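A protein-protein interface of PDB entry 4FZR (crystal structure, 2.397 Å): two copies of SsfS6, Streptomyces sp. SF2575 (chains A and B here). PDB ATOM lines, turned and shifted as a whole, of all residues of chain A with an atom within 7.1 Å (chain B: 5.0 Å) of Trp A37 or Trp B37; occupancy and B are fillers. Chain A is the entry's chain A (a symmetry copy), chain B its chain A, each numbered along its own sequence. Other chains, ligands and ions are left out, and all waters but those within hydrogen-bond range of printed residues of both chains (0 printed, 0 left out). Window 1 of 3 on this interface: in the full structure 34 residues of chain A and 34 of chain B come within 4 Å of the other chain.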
ATOM      1  N   LEU A  32     -21.776  17.258 -12.885  1.00  0.00           N
ATOM      2  CA  LEU A  32     -20.907  16.119 -12.589  1.00  0.00           C
ATOM      3  C   LEU A  32     -19.580  16.212 -13.335  1.00  0.00           C
ATOM      4  O   LEU A  32     -18.672  15.417 -13.104  1.00  0.00           O
ATOM      5  CB  LEU A  32     -21.598  14.805 -12.954  1.00  0.00           C
ATOM      6  CG  LEU A  32     -22.795  14.402 -12.092  1.00  0.00           C
ATOM      7  CD1 LEU A  32     -23.482  13.191 -12.693  1.00  0.00           C
ATOM      8  CD2 LEU A  32     -22.371  14.117 -10.653  1.00  0.00           C
ATOM      9  N   VAL A  33     -19.472  17.192 -14.225  1.00  0.00           N
ATOM     10  CA  VAL A  33     -18.297  17.315 -15.079  1.00  0.00           C
ATOM     11  C   VAL A  33     -17.007  17.592 -14.300  1.00  0.00           C
ATOM     12  O   VAL A  33     -15.981  16.973 -14.568  1.00  0.00           O
ATOM     13  CB  VAL A  33     -18.513  18.398 -16.163  1.00  0.00           C
ATOM     14  CG1 VAL A  33     -17.194  18.788 -16.804  1.00  0.00           C
ATOM     15  CG2 VAL A  33     -19.503  17.909 -17.214  1.00  0.00           C
ATOM     16  N   PRO A  34     -17.045  18.529 -13.338  1.00  0.00           N
ATOM     17  CA  PRO A  34     -15.789  18.835 -12.637  1.00  0.00           C
ATOM     18  C   PRO A  34     -15.252  17.684 -11.776  1.00  0.00           C
ATOM     19  O   PRO A  34     -14.037  17.502 -11.709  1.00  0.00           O
ATOM     20  CB  PRO A  34     -16.159  20.048 -11.774  1.00  0.00           C
ATOM     21  CG  PRO A  34     -17.312  20.676 -12.495  1.00  0.00           C
ATOM     22  CD  PRO A  34     -18.095  19.513 -13.022  1.00  0.00           C
ATOM     23  N   LEU A  35     -16.131  16.922 -11.135  1.00  0.00           N
ATOM     24  CA  LEU A  35     -15.688  15.769 -10.362  1.00  0.00           C
ATOM     25  C   LEU A  35     -15.153  14.686 -11.297  1.00  0.00           C
ATOM     26  O   LEU A  35     -14.177  14.004 -10.978  1.00  0.00           O
ATOM     27  CB  LEU A  35     -16.831  15.212  -9.509  1.00  0.00           C
ATOM     28  CG  LEU A  35     -16.468  14.041  -8.589  1.00  0.00           C
ATOM     29  CD1 LEU A  35     -15.252  14.359  -7.727  1.00  0.00           C
ATOM     30  CD2 LEU A  35     -17.654  13.663  -7.709  1.00  0.00           C
ATOM     31  N   SER A  36     -15.792  14.545 -12.456  1.00  0.00           N
ATOM     32  CA  SER A  36     -15.387  13.562 -13.458  1.00  0.00           C
ATOM     33  C   SER A  36     -13.992  13.855 -13.989  1.00  0.00           C
ATOM     34  O   SER A  36     -13.192  12.944 -14.196  1.00  0.00           O
ATOM     35  CB  SER A  36     -16.372  13.552 -14.626  1.00  0.00           C
ATOM     36  OG  SER A  36     -17.580  12.900 -14.276  1.00  0.00           O
ATOM     37  N   TRP A  37     -13.711  15.131 -14.225  1.00  0.00           N
ATOM     38  CA  TRP A  37     -12.390  15.538 -14.686  1.00  0.00           C
ATOM     39  C   TRP A  37     -11.353  15.486 -13.561  1.00  0.00           C
ATOM     40  O   TRP A  37     -10.159  15.319 -13.819  1.00  0.00           O
ATOM     41  CB  TRP A  37     -12.435  16.939 -15.301  1.00  0.00           C
ATOM     42  CG  TRP A  37     -12.418  16.913 -16.800  1.00  0.00           C
ATOM     43  CD1 TRP A  37     -13.431  17.277 -17.641  1.00  0.00           C
ATOM     44  CD2 TRP A  37     -11.335  16.486 -17.636  1.00  0.00           C
ATOM     45  NE1 TRP A  37     -13.041  17.110 -18.950  1.00  0.00           N
ATOM     46  CE2 TRP A  37     -11.760  16.626 -18.974  1.00  0.00           C
ATOM     47  CE3 TRP A  37     -10.044  16.005 -17.384  1.00  0.00           C
ATOM     48  CZ2 TRP A  37     -10.941  16.301 -20.057  1.00  0.00           C
ATOM     49  CZ3 TRP A  37      -9.231  15.683 -18.462  1.00  0.00           C
ATOM     50  CH2 TRP A  37      -9.684  15.832 -19.781  1.00  0.00           C
ATOM     51  N   ALA A  38     -11.811  15.641 -12.322  1.00  0.00           N
ATOM     52  CA  ALA A  38     -10.928  15.546 -11.166  1.00  0.00           C
ATOM     53  C   ALA A  38     -10.418  14.116 -11.043  1.00  0.00           C
ATOM     54  O   ALA A  38      -9.252  13.883 -10.722  1.00  0.00           O
ATOM     55  CB  ALA A  38     -11.663  15.960  -9.895  1.00  0.00           C
ATOM     56  N   LEU A  39     -11.304  13.162 -11.305  1.00  0.00           N
ATOM     57  CA  LEU A  39     -10.933  11.753 -11.313  1.00  0.00           C
ATOM     58  C   LEU A  39      -9.937  11.474 -12.430  1.00  0.00           C
ATOM     59  O   LEU A  39      -8.902  10.842 -12.216  1.00  0.00           O
ATOM     60  CB  LEU A  39     -12.176  10.877 -11.494  1.00  0.00           C
ATOM     61  CG  LEU A  39     -13.182  10.905 -10.340  1.00  0.00           C
ATOM     62  CD1 LEU A  39     -14.469  10.172 -10.713  1.00  0.00           C
ATOM     63  CD2 LEU A  39     -12.568  10.315  -9.076  1.00  0.00           C
ATOM     64  N   ARG A  40     -10.255  11.953 -13.625  1.00  0.00           N
ATOM     65  CA  ARG A  40      -9.404  11.734 -14.783  1.00  0.00           C
ATOM     66  C   ARG A  40      -8.039  12.381 -14.573  1.00  0.00           C
ATOM     67  O   ARG A  40      -7.013  11.841 -14.982  1.00  0.00           O
ATOM     68  CB  ARG A  40     -10.080  12.297 -16.030  1.00  0.00           C
ATOM     69  CG  ARG A  40      -9.615  11.671 -17.327  1.00  0.00           C
ATOM     70  CD  ARG A  40     -10.567  12.025 -18.456  1.00  0.00           C
ATOM     71  NE  ARG A  40     -10.079  11.575 -19.757  1.00  0.00           N
ATOM     72  CZ  ARG A  40     -10.541  12.015 -20.924  1.00  0.00           C
ATOM     73  NH1 ARG A  40     -11.503  12.930 -20.966  1.00  0.00           N
ATOM     74  NH2 ARG A  40     -10.035  11.546 -22.056  1.00  0.00           N
ATOM     75  N   ALA A  41      -8.024  13.541 -13.924  1.00  0.00           N
ATOM     76  CA  ALA A  41      -6.776  14.236 -13.643  1.00  0.00           C
ATOM     77  C   ALA A  41      -5.920  13.437 -12.665  1.00  0.00           C
ATOM     78  O   ALA A  41      -4.693  13.555 -12.657  1.00  0.00           O
ATOM     79  CB  ALA A  41      -7.054  15.611 -13.083  1.00  0.00           C
ATOM     80  N   ALA A  42      -6.576  12.628 -11.839  1.00  0.00           N
ATOM     81  CA  ALA A  42      -5.880  11.788 -10.872  1.00  0.00           C
ATOM     82  C   ALA A  42      -5.559  10.415 -11.456  1.00  0.00           C
ATOM     83  O   ALA A  42      -5.330   9.458 -10.718  1.00  0.00           O
ATOM     84  CB  ALA A  42      -6.711  11.641  -9.609  1.00  0.00           C
ATOM     85  N   GLY A  43      -5.562  10.320 -12.783  1.00  0.00           N
ATOM     86  CA  GLY A  43      -5.088   9.128 -13.459  1.00  0.00           C
ATOM     87  C   GLY A  43      -6.131   8.044 -13.651  1.00  0.00           C
ATOM     88  O   GLY A  43      -5.842   7.003 -14.241  1.00  0.00           O
ATOM     89  N   VAL A  46     -12.514   7.216 -16.859  1.00  0.00           N
ATOM     90  CA  VAL A  46     -13.889   7.678 -16.693  1.00  0.00           C
ATOM     91  C   VAL A  46     -14.724   7.484 -17.956  1.00  0.00           C
ATOM     92  O   VAL A  46     -14.259   7.719 -19.070  1.00  0.00           O
ATOM     93  CB  VAL A  46     -13.932   9.171 -16.283  1.00  0.00           C
ATOM     94  CG1 VAL A  46     -15.345   9.733 -16.408  1.00  0.00           C
ATOM     95  CG2 VAL A  46     -13.406   9.346 -14.865  1.00  0.00           C
ATOM     96  N   VAL A  58     -21.808  15.909 -22.999  1.00  0.00           N
ATOM     97  CA  VAL A  58     -20.754  15.142 -22.349  1.00  0.00           C
ATOM     98  C   VAL A  58     -19.430  15.293 -23.096  1.00  0.00           C
ATOM     99  O   VAL A  58     -18.397  15.564 -22.488  1.00  0.00           O
ATOM    100  CB  VAL A  58     -21.135  13.652 -22.245  1.00  0.00           C
ATOM    101  CG1 VAL A  58     -19.950  12.820 -21.753  1.00  0.00           C
ATOM    102  CG2 VAL A  58     -22.363  13.483 -21.339  1.00  0.00           C
ATOM    103  N   ALA A  61     -17.812  18.661 -22.946  1.00  0.00           N
ATOM    104  CA  ALA A  61     -17.075  18.894 -21.706  1.00  0.00           C
ATOM    105  C   ALA A  61     -15.724  18.177 -21.731  1.00  0.00           C
ATOM    106  O   ALA A  61     -14.977  18.208 -20.751  1.00  0.00           O
ATOM    107  CB  ALA A  61     -17.902  18.420 -20.511  1.00  0.00           C
ATOM    108  N   GLY A  62     -15.423  17.523 -22.850  1.00  0.00           N
ATOM    109  CA  GLY A  62     -14.150  16.853 -23.036  1.00  0.00           C
ATOM    110  C   GLY A  62     -14.116  15.470 -22.420  1.00  0.00           C
ATOM    111  O   GLY A  62     -13.040  14.945 -22.145  1.00  0.00           O
ATOM    112  N   LEU A  63     -15.288  14.875 -22.216  1.00  0.00           N
ATOM    113  CA  LEU A  63     -15.376  13.579 -21.545  1.00  0.00           C
ATOM    114  C   LEU A  63     -15.890  12.466 -22.466  1.00  0.00           C
ATOM    115  O   LEU A  63     -16.642  12.723 -23.406  1.00  0.00           O
ATOM    116  CB  LEU A  63     -16.264  13.686 -20.298  1.00  0.00           C
ATOM    117  CG  LEU A  63     -15.732  14.580 -19.171  1.00  0.00           C
ATOM    118  CD1 LEU A  63     -16.806  14.821 -18.124  1.00  0.00           C
ATOM    119  CD2 LEU A  63     -14.492  13.973 -18.524  1.00  0.00           C
ATOM    120  N   PRO A  64     -15.472  11.217 -22.204  1.00  0.00           N
ATOM    121  CA  PRO A  64     -15.960  10.055 -22.960  1.00  0.00           C
ATOM    122  C   PRO A  64     -17.440   9.783 -22.708  1.00  0.00           C
ATOM    123  O   PRO A  64     -17.885   9.897 -21.570  1.00  0.00           O
ATOM    124  CB  PRO A  64     -15.109   8.898 -22.418  1.00  0.00           C
ATOM    125  CG  PRO A  64     -13.929   9.541 -21.776  1.00  0.00           C
ATOM    126  CD  PRO A  64     -14.430  10.838 -21.234  1.00  0.00           C
ATOM    127  N   LEU A 128     -20.156   6.704 -10.092  1.00  0.00           N
ATOM    128  CA  LEU A 128     -20.411   8.067  -9.638  1.00  0.00           C
ATOM    129  C   LEU A 128     -21.721   8.555 -10.247  1.00  0.00           C
ATOM    130  O   LEU A 128     -21.963   8.379 -11.443  1.00  0.00           O
ATOM    131  CB  LEU A 128     -19.262   8.993 -10.036  1.00  0.00           C
ATOM    132  CG  LEU A 128     -19.540  10.502 -10.023  1.00  0.00           C
ATOM    133  CD1 LEU A 128     -19.884  10.993  -8.625  1.00  0.00           C
ATOM    134  CD2 LEU A 128     -18.345  11.264 -10.582  1.00  0.00           C
ATOM    135  N   VAL A 208     -17.598  23.701  -8.010  1.00  0.00           N
ATOM    136  CA  VAL A 208     -16.885  24.306  -9.125  1.00  0.00           C
ATOM    137  C   VAL A 208     -17.851  24.394 -10.307  1.00  0.00           C
ATOM    138  O   VAL A 208     -18.358  23.374 -10.778  1.00  0.00           O
ATOM    139  CB  VAL A 208     -15.631  23.496  -9.503  1.00  0.00           C
ATOM    140  CG1 VAL A 208     -14.997  24.046 -10.779  1.00  0.00           C
ATOM    141  CG2 VAL A 208     -14.629  23.503  -8.350  1.00  0.00           C
ATOM    142  N   PRO A 209     -18.134  25.619 -10.773  1.00  0.00           N
ATOM    143  CA  PRO A 209     -19.137  25.782 -11.833  1.00  0.00           C
ATOM    144  C   PRO A 209     -18.716  25.192 -13.177  1.00  0.00           C
ATOM    145  O   PRO A 209     -17.582  25.398 -13.619  1.00  0.00           O
ATOM    146  CB  PRO A 209     -19.279  27.307 -11.957  1.00  0.00           C
ATOM    147  CG  PRO A 209     -18.704  27.867 -10.692  1.00  0.00           C
ATOM    148  CD  PRO A 209     -17.639  26.914 -10.275  1.00  0.00           C
ATOM    149  N   TYR A 210     -19.622  24.453 -13.810  1.00  0.00           N
ATOM    150  CA  TYR A 210     -19.480  24.142 -15.224  1.00  0.00           C
ATOM    151  C   TYR A 210     -20.799  24.370 -15.951  1.00  0.00           C
ATOM    152  O   TYR A 210     -21.760  23.624 -15.773  1.00  0.00           O
ATOM    153  CB  TYR A 210     -19.006  22.708 -15.454  1.00  0.00           C
ATOM    154  CG  TYR A 210     -18.856  22.401 -16.926  1.00  0.00           C
ATOM    155  CD1 TYR A 210     -17.810  22.947 -17.662  1.00  0.00           C
ATOM    156  CD2 TYR A 210     -19.771  21.594 -17.586  1.00  0.00           C
ATOM    157  CE1 TYR A 210     -17.675  22.689 -19.009  1.00  0.00           C
ATOM    158  CE2 TYR A 210     -19.643  21.327 -18.936  1.00  0.00           C
ATOM    159  CZ  TYR A 210     -18.592  21.876 -19.641  1.00  0.00           C
ATOM    160  OH  TYR A 210     -18.463  21.617 -20.984  1.00  0.00           O
ATOM    161  N   VAL A 392     -11.489  13.494  -4.454  1.00  0.00           N
ATOM    162  CA  VAL A 392     -10.955  12.335  -5.156  1.00  0.00           C
ATOM    163  C   VAL A 392     -10.002  11.566  -4.243  1.00  0.00           C
ATOM    164  O   VAL A 392     -10.006  10.335  -4.225  1.00  0.00           O
ATOM    165  CB  VAL A 392     -10.234  12.729  -6.464  1.00  0.00           C
ATOM    166  CG1 VAL A 392      -9.500  11.531  -7.048  1.00  0.00           C
ATOM    167  CG2 VAL A 392     -11.228  13.284  -7.477  1.00  0.00           C
ATOM    168  N   VAL B  33      -4.614  19.979 -21.857  1.00  0.00           N
ATOM    169  CA  VAL B  33      -5.979  19.923 -21.350  1.00  0.00           C
ATOM    170  C   VAL B  33      -6.091  19.234 -19.985  1.00  0.00           C
ATOM    171  O   VAL B  33      -6.777  19.734 -19.098  1.00  0.00           O
ATOM    172  CB  VAL B  33      -6.922  19.243 -22.373  1.00  0.00           C
ATOM    173  CG1 VAL B  33      -8.233  18.850 -21.719  1.00  0.00           C
ATOM    174  CG2 VAL B  33      -7.165  20.162 -23.564  1.00  0.00           C
ATOM    175  N   PRO B  34      -5.428  18.079 -19.809  1.00  0.00           N
ATOM    176  CA  PRO B  34      -5.590  17.392 -18.520  1.00  0.00           C
ATOM    177  C   PRO B  34      -4.997  18.148 -17.325  1.00  0.00           C
ATOM    178  O   PRO B  34      -5.579  18.110 -16.242  1.00  0.00           O
ATOM    179  CB  PRO B  34      -4.869  16.057 -18.746  1.00  0.00           C
ATOM    180  CG  PRO B  34      -4.927  15.851 -20.228  1.00  0.00           C
ATOM    181  CD  PRO B  34      -4.747  17.224 -20.799  1.00  0.00           C
ATOM    182  N   LEU B  35      -3.868  18.823 -17.512  1.00  0.00           N
ATOM    183  CA  LEU B  35      -3.294  19.623 -16.436  1.00  0.00           C
ATOM    184  C   LEU B  35      -4.186  20.828 -16.148  1.00  0.00           C
ATOM    185  O   LEU B  35      -4.352  21.229 -14.995  1.00  0.00           O
ATOM    186  CB  LEU B  35      -1.879  20.084 -16.794  1.00  0.00           C
ATOM    187  CG  LEU B  35      -1.138  20.870 -15.707  1.00  0.00           C
ATOM    188  CD1 LEU B  35      -1.148  20.131 -14.374  1.00  0.00           C
ATOM    189  CD2 LEU B  35       0.294  21.162 -16.137  1.00  0.00           C
ATOM    190  N   SER B  36      -4.764  21.395 -17.205  1.00  0.00           N
ATOM    191  CA  SER B  36      -5.654  22.547 -17.085  1.00  0.00           C
ATOM    192  C   SER B  36      -6.902  22.202 -16.286  1.00  0.00           C
ATOM    193  O   SER B  36      -7.367  22.996 -15.471  1.00  0.00           O
ATOM    194  CB  SER B  36      -6.071  23.046 -18.469  1.00  0.00           C
ATOM    195  OG  SER B  36      -5.018  23.752 -19.100  1.00  0.00           O
ATOM    196  N   TRP B  37      -7.451  21.020 -16.537  1.00  0.00           N
ATOM    197  CA  TRP B  37      -8.618  20.559 -15.797  1.00  0.00           C
ATOM    198  C   TRP B  37      -8.255  20.123 -14.375  1.00  0.00           C
ATOM    199  O   TRP B  37      -9.095  20.166 -13.475  1.00  0.00           O
ATOM    200  CB  TRP B  37      -9.318  19.418 -16.539  1.00  0.00           C
ATOM    201  CG  TRP B  37     -10.555  19.869 -17.257  1.00  0.00           C
ATOM    202  CD1 TRP B  37     -10.747  19.926 -18.609  1.00  0.00           C
ATOM    203  CD2 TRP B  37     -11.769  20.342 -16.658  1.00  0.00           C
ATOM    204  NE1 TRP B  37     -12.009  20.397 -18.887  1.00  0.00           N
ATOM    205  CE2 TRP B  37     -12.656  20.659 -17.708  1.00  0.00           C
ATOM    206  CE3 TRP B  37     -12.194  20.522 -15.336  1.00  0.00           C
ATOM    207  CZ2 TRP B  37     -13.943  21.149 -17.477  1.00  0.00           C
ATOM    208  CZ3 TRP B  37     -13.474  21.006 -15.108  1.00  0.00           C
ATOM    209  CH2 TRP B  37     -14.332  21.315 -16.175  1.00  0.00           C
ATOM    210  N   ALA B  38      -7.012  19.694 -14.184  1.00  0.00           N
ATOM    211  CA  ALA B  38      -6.531  19.314 -12.861  1.00  0.00           C
ATOM    212  C   ALA B  38      -6.485  20.550 -11.972  1.00  0.00           C
ATOM    213  O   ALA B  38      -6.825  20.495 -10.789  1.00  0.00           O
ATOM    214  CB  ALA B  38      -5.149  18.674 -12.956  1.00  0.00           C
ATOM    215  N   LEU B  39      -6.063  21.667 -12.555  1.00  0.00           N
ATOM    216  CA  LEU B  39      -6.052  22.942 -11.852  1.00  0.00           C
ATOM    217  C   LEU B  39      -7.471  23.368 -11.505  1.00  0.00           C
ATOM    218  O   LEU B  39      -7.764  23.741 -10.368  1.00  0.00           O
ATOM    219  CB  LEU B  39      -5.380  24.017 -12.710  1.00  0.00           C
ATOM    220  CG  LEU B  39      -3.886  23.818 -12.975  1.00  0.00           C
ATOM    221  CD1 LEU B  39      -3.370  24.821 -14.006  1.00  0.00           C
ATOM    222  CD2 LEU B  39      -3.091  23.917 -11.677  1.00  0.00           C
ATOM    223  N   ARG B  40      -8.354  23.308 -12.494  1.00  0.00           N
ATOM    224  CA  ARG B  40      -9.737  23.713 -12.304  1.00  0.00           C
ATOM    225  C   ARG B  40     -10.416  22.825 -11.264  1.00  0.00           C
ATOM    226  O   ARG B  40     -11.229  23.293 -10.470  1.00  0.00           O
ATOM    227  CB  ARG B  40     -10.479  23.643 -13.635  1.00  0.00           C
ATOM    228  CG  ARG B  40     -11.700  24.533 -13.715  1.00  0.00           C
ATOM    229  CD  ARG B  40     -12.160  24.673 -15.155  1.00  0.00           C
ATOM    230  NE  ARG B  40     -13.426  25.392 -15.268  1.00  0.00           N
ATOM    231  CZ  ARG B  40     -14.200  25.384 -16.350  1.00  0.00           C
ATOM    232  NH1 ARG B  40     -13.851  24.683 -17.422  1.00  0.00           N
ATOM    233  NH2 ARG B  40     -15.333  26.072 -16.359  1.00  0.00           N
ATOM    234  N   ALA B  41     -10.073  21.541 -11.264  1.00  0.00           N
ATOM    235  CA  ALA B  41     -10.637  20.607 -10.299  1.00  0.00           C
ATOM    236  C   ALA B  41     -10.177  20.948  -8.885  1.00  0.00           C
ATOM    237  O   ALA B  41     -10.862  20.641  -7.907  1.00  0.00           O
ATOM    238  CB  ALA B  41     -10.240  19.192 -10.645  1.00  0.00           C
ATOM    239  N   ALA B  42      -9.012  21.580  -8.784  1.00  0.00           N
ATOM    240  CA  ALA B  42      -8.468  21.987  -7.495  1.00  0.00           C
ATOM    241  C   ALA B  42      -8.907  23.401  -7.127  1.00  0.00           C
ATOM    242  O   ALA B  42      -8.276  24.059  -6.300  1.00  0.00           O
ATOM    243  CB  ALA B  42      -6.951  21.895  -7.511  1.00  0.00           C
ATOM    244  N   ALA B  61     -12.918  20.827 -25.221  1.00  0.00           N
ATOM    245  CA  ALA B  61     -12.340  20.136 -24.071  1.00  0.00           C
ATOM    246  C   ALA B  61     -12.989  20.607 -22.769  1.00  0.00           C
ATOM    247  O   ALA B  61     -12.599  20.180 -21.680  1.00  0.00           O
ATOM    248  CB  ALA B  61     -10.830  20.372 -24.024  1.00  0.00           C
ATOM    249  N   GLY B  62     -13.969  21.499 -22.887  1.00  0.00           N
ATOM    250  CA  GLY B  62     -14.716  21.984 -21.741  1.00  0.00           C
ATOM    251  C   GLY B  62     -14.011  23.110 -21.013  1.00  0.00           C
ATOM    252  O   GLY B  62     -14.292  23.358 -19.843  1.00  0.00           O
ATOM    253  N   LEU B  63     -13.106  23.799 -21.705  1.00  0.00           N
ATOM    254  CA  LEU B  63     -12.303  24.845 -21.074  1.00  0.00           C
ATOM    255  C   LEU B  63     -12.602  26.242 -21.633  1.00  0.00           C
ATOM    256  O   LEU B  63     -13.002  26.386 -22.787  1.00  0.00           O
ATOM    257  CB  LEU B  63     -10.809  24.527 -21.219  1.00  0.00           C
ATOM    258  CG  LEU B  63     -10.316  23.275 -20.481  1.00  0.00           C
ATOM    259  CD1 LEU B  63      -8.906  22.917 -20.915  1.00  0.00           C
ATOM    260  CD2 LEU B  63     -10.370  23.469 -18.970  1.00  0.00           C
ATOM    261  N   TYR B 210      -5.334  13.022 -23.855  1.00  0.00           N
ATOM    262  CA  TYR B 210      -6.524  13.698 -24.348  1.00  0.00           C
ATOM    263  C   TYR B 210      -6.434  13.898 -25.856  1.00  0.00           C
ATOM    264  O   TYR B 210      -5.642  14.704 -26.342  1.00  0.00           O
ATOM    265  CB  TYR B 210      -6.747  15.044 -23.662  1.00  0.00           C
ATOM    266  CG  TYR B 210      -7.990  15.732 -24.177  1.00  0.00           C
ATOM    267  CD1 TYR B 210      -9.255  15.262 -23.838  1.00  0.00           C
ATOM    268  CD2 TYR B 210      -7.903  16.828 -25.024  1.00  0.00           C
ATOM    269  CE1 TYR B 210     -10.394  15.871 -24.319  1.00  0.00           C
ATOM    270  CE2 TYR B 210      -9.039  17.447 -25.509  1.00  0.00           C
ATOM    271  CZ  TYR B 210     -10.282  16.964 -25.152  1.00  0.00           C
ATOM    272  OH  TYR B 210     -11.415  17.574 -25.634  1.00  0.00           O
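Trp A37 touches just these residues of chain B: Val B33 (3.9 Å) and Trp B37 (3.4 Å). Printed residues of chain B within 4 Å of Tyr A210: Gly B62. Printed residues of chain A within 4 Å of Val B33: Trp A37 (3.9 Å). Pro A64 touches none of the printed residues of chain B.
Trp B37 touches Val A33 (CH2 to CG1, 3.9 Å). CG1 of Val B33 touches CH2 of Trp A37 (3.9 Å). Ala A38 touches Ala B41 (CB to CB, 3.6 Å). Ala A41 touches Ala B38 (CB to CB, 3.6 Å). CA of Ala A61 touches CA of Gly B62, 3.9 Å away. Gly A62 touches Ala B61 (CA to CA, 3.9 Å). Gly A62 touches Tyr B210 (O to CE1, 3.5 Å). O of Arg B40 touches CG1 of Val A208, 3.9 Å away. O of Pro A209 touches NH2 of Arg B40, 3.6 Å away. CE1 of Tyr A210 touches O of Gly B62, at 3.5 Å.
Val A33 touches Trp B37, and with the chains exchanged Trp A37 touches Val B33. Trp B37 touches its own counterpart, Trp A37. Ala A38 touches Ala B41, and with the chains exchanged Ala A41 touches Ala B38. Ala A61 touches its own counterpart, Ala B61. Positions printed for both chains: 33, 34, 35, 36, 37, 38, 39, 40, 41, 42, 61, 62, 63 and 210. Of the 12 pairs that touch across the chains among the printed residues, 10 have their exchanged pair printed and touching as well.
Of the 14 printed residues of chain B, 8 touch a printed residue of chain A. Printed residues of chain B that touch a printed residue of chain A: Val B33, Trp B37, Ala B38, Arg B40, Ala B41, Ala B61, Gly B62 and Tyr B210. Hydrophobic or aromatic side chains of chain B within 4 Å of the printed part of chain A: Val B33, Trp B37, Ala B38, Ala B41 and Tyr B210. Along chain B the printed residues that touch a printed residue of chain A span positions 33 to 210. Of the 23 printed residues of chain A, 9 touch a printed residue of chain B. Printed residues of chain A that touch a printed residue of chain B: Val A33, Trp A37, Ala A38, Ala A41, Ala A61, Gly A62, Val A208, Pro A209 and Tyr A210. Hydrophobic or aromatic side chains of chain A that line the printed part of chain B: Val A33, Trp A37, Ala A38, Ala A41, Val A208 and Tyr A210. Among the printed residues, 12 pairs touch across the chains.
The indole nitrogen (NE1) of Trp B37 lies close to the indole nitrogen (NE1) of Trp A37, at 3.4 Å. The backbone carbonyl oxygen (O) of Ala B61 lies close to the backbone carbonyl oxygen (O) of Ala A61, at 3.2 Å.
The indole nitrogen (NE1) of Trp B37 is in hydrogen-bond range of the backbone carbonyl oxygen (O) of Ala B61. The backbone carbonyl oxygen (O) of Gly B62 lies within hydrogen-bond range of the guanidinium group (NH1) of Arg B40. The indole nitrogen (NE1) of Trp A37 lies within hydrogen-bond range of the backbone carbonyl oxygen (O) of Ala A61 (2.9 Å). The guanidinium group of Arg A40 sits at hydrogen-bond distance from the backbone carbonyl oxygen of Gly A62, 2.8 Å away.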
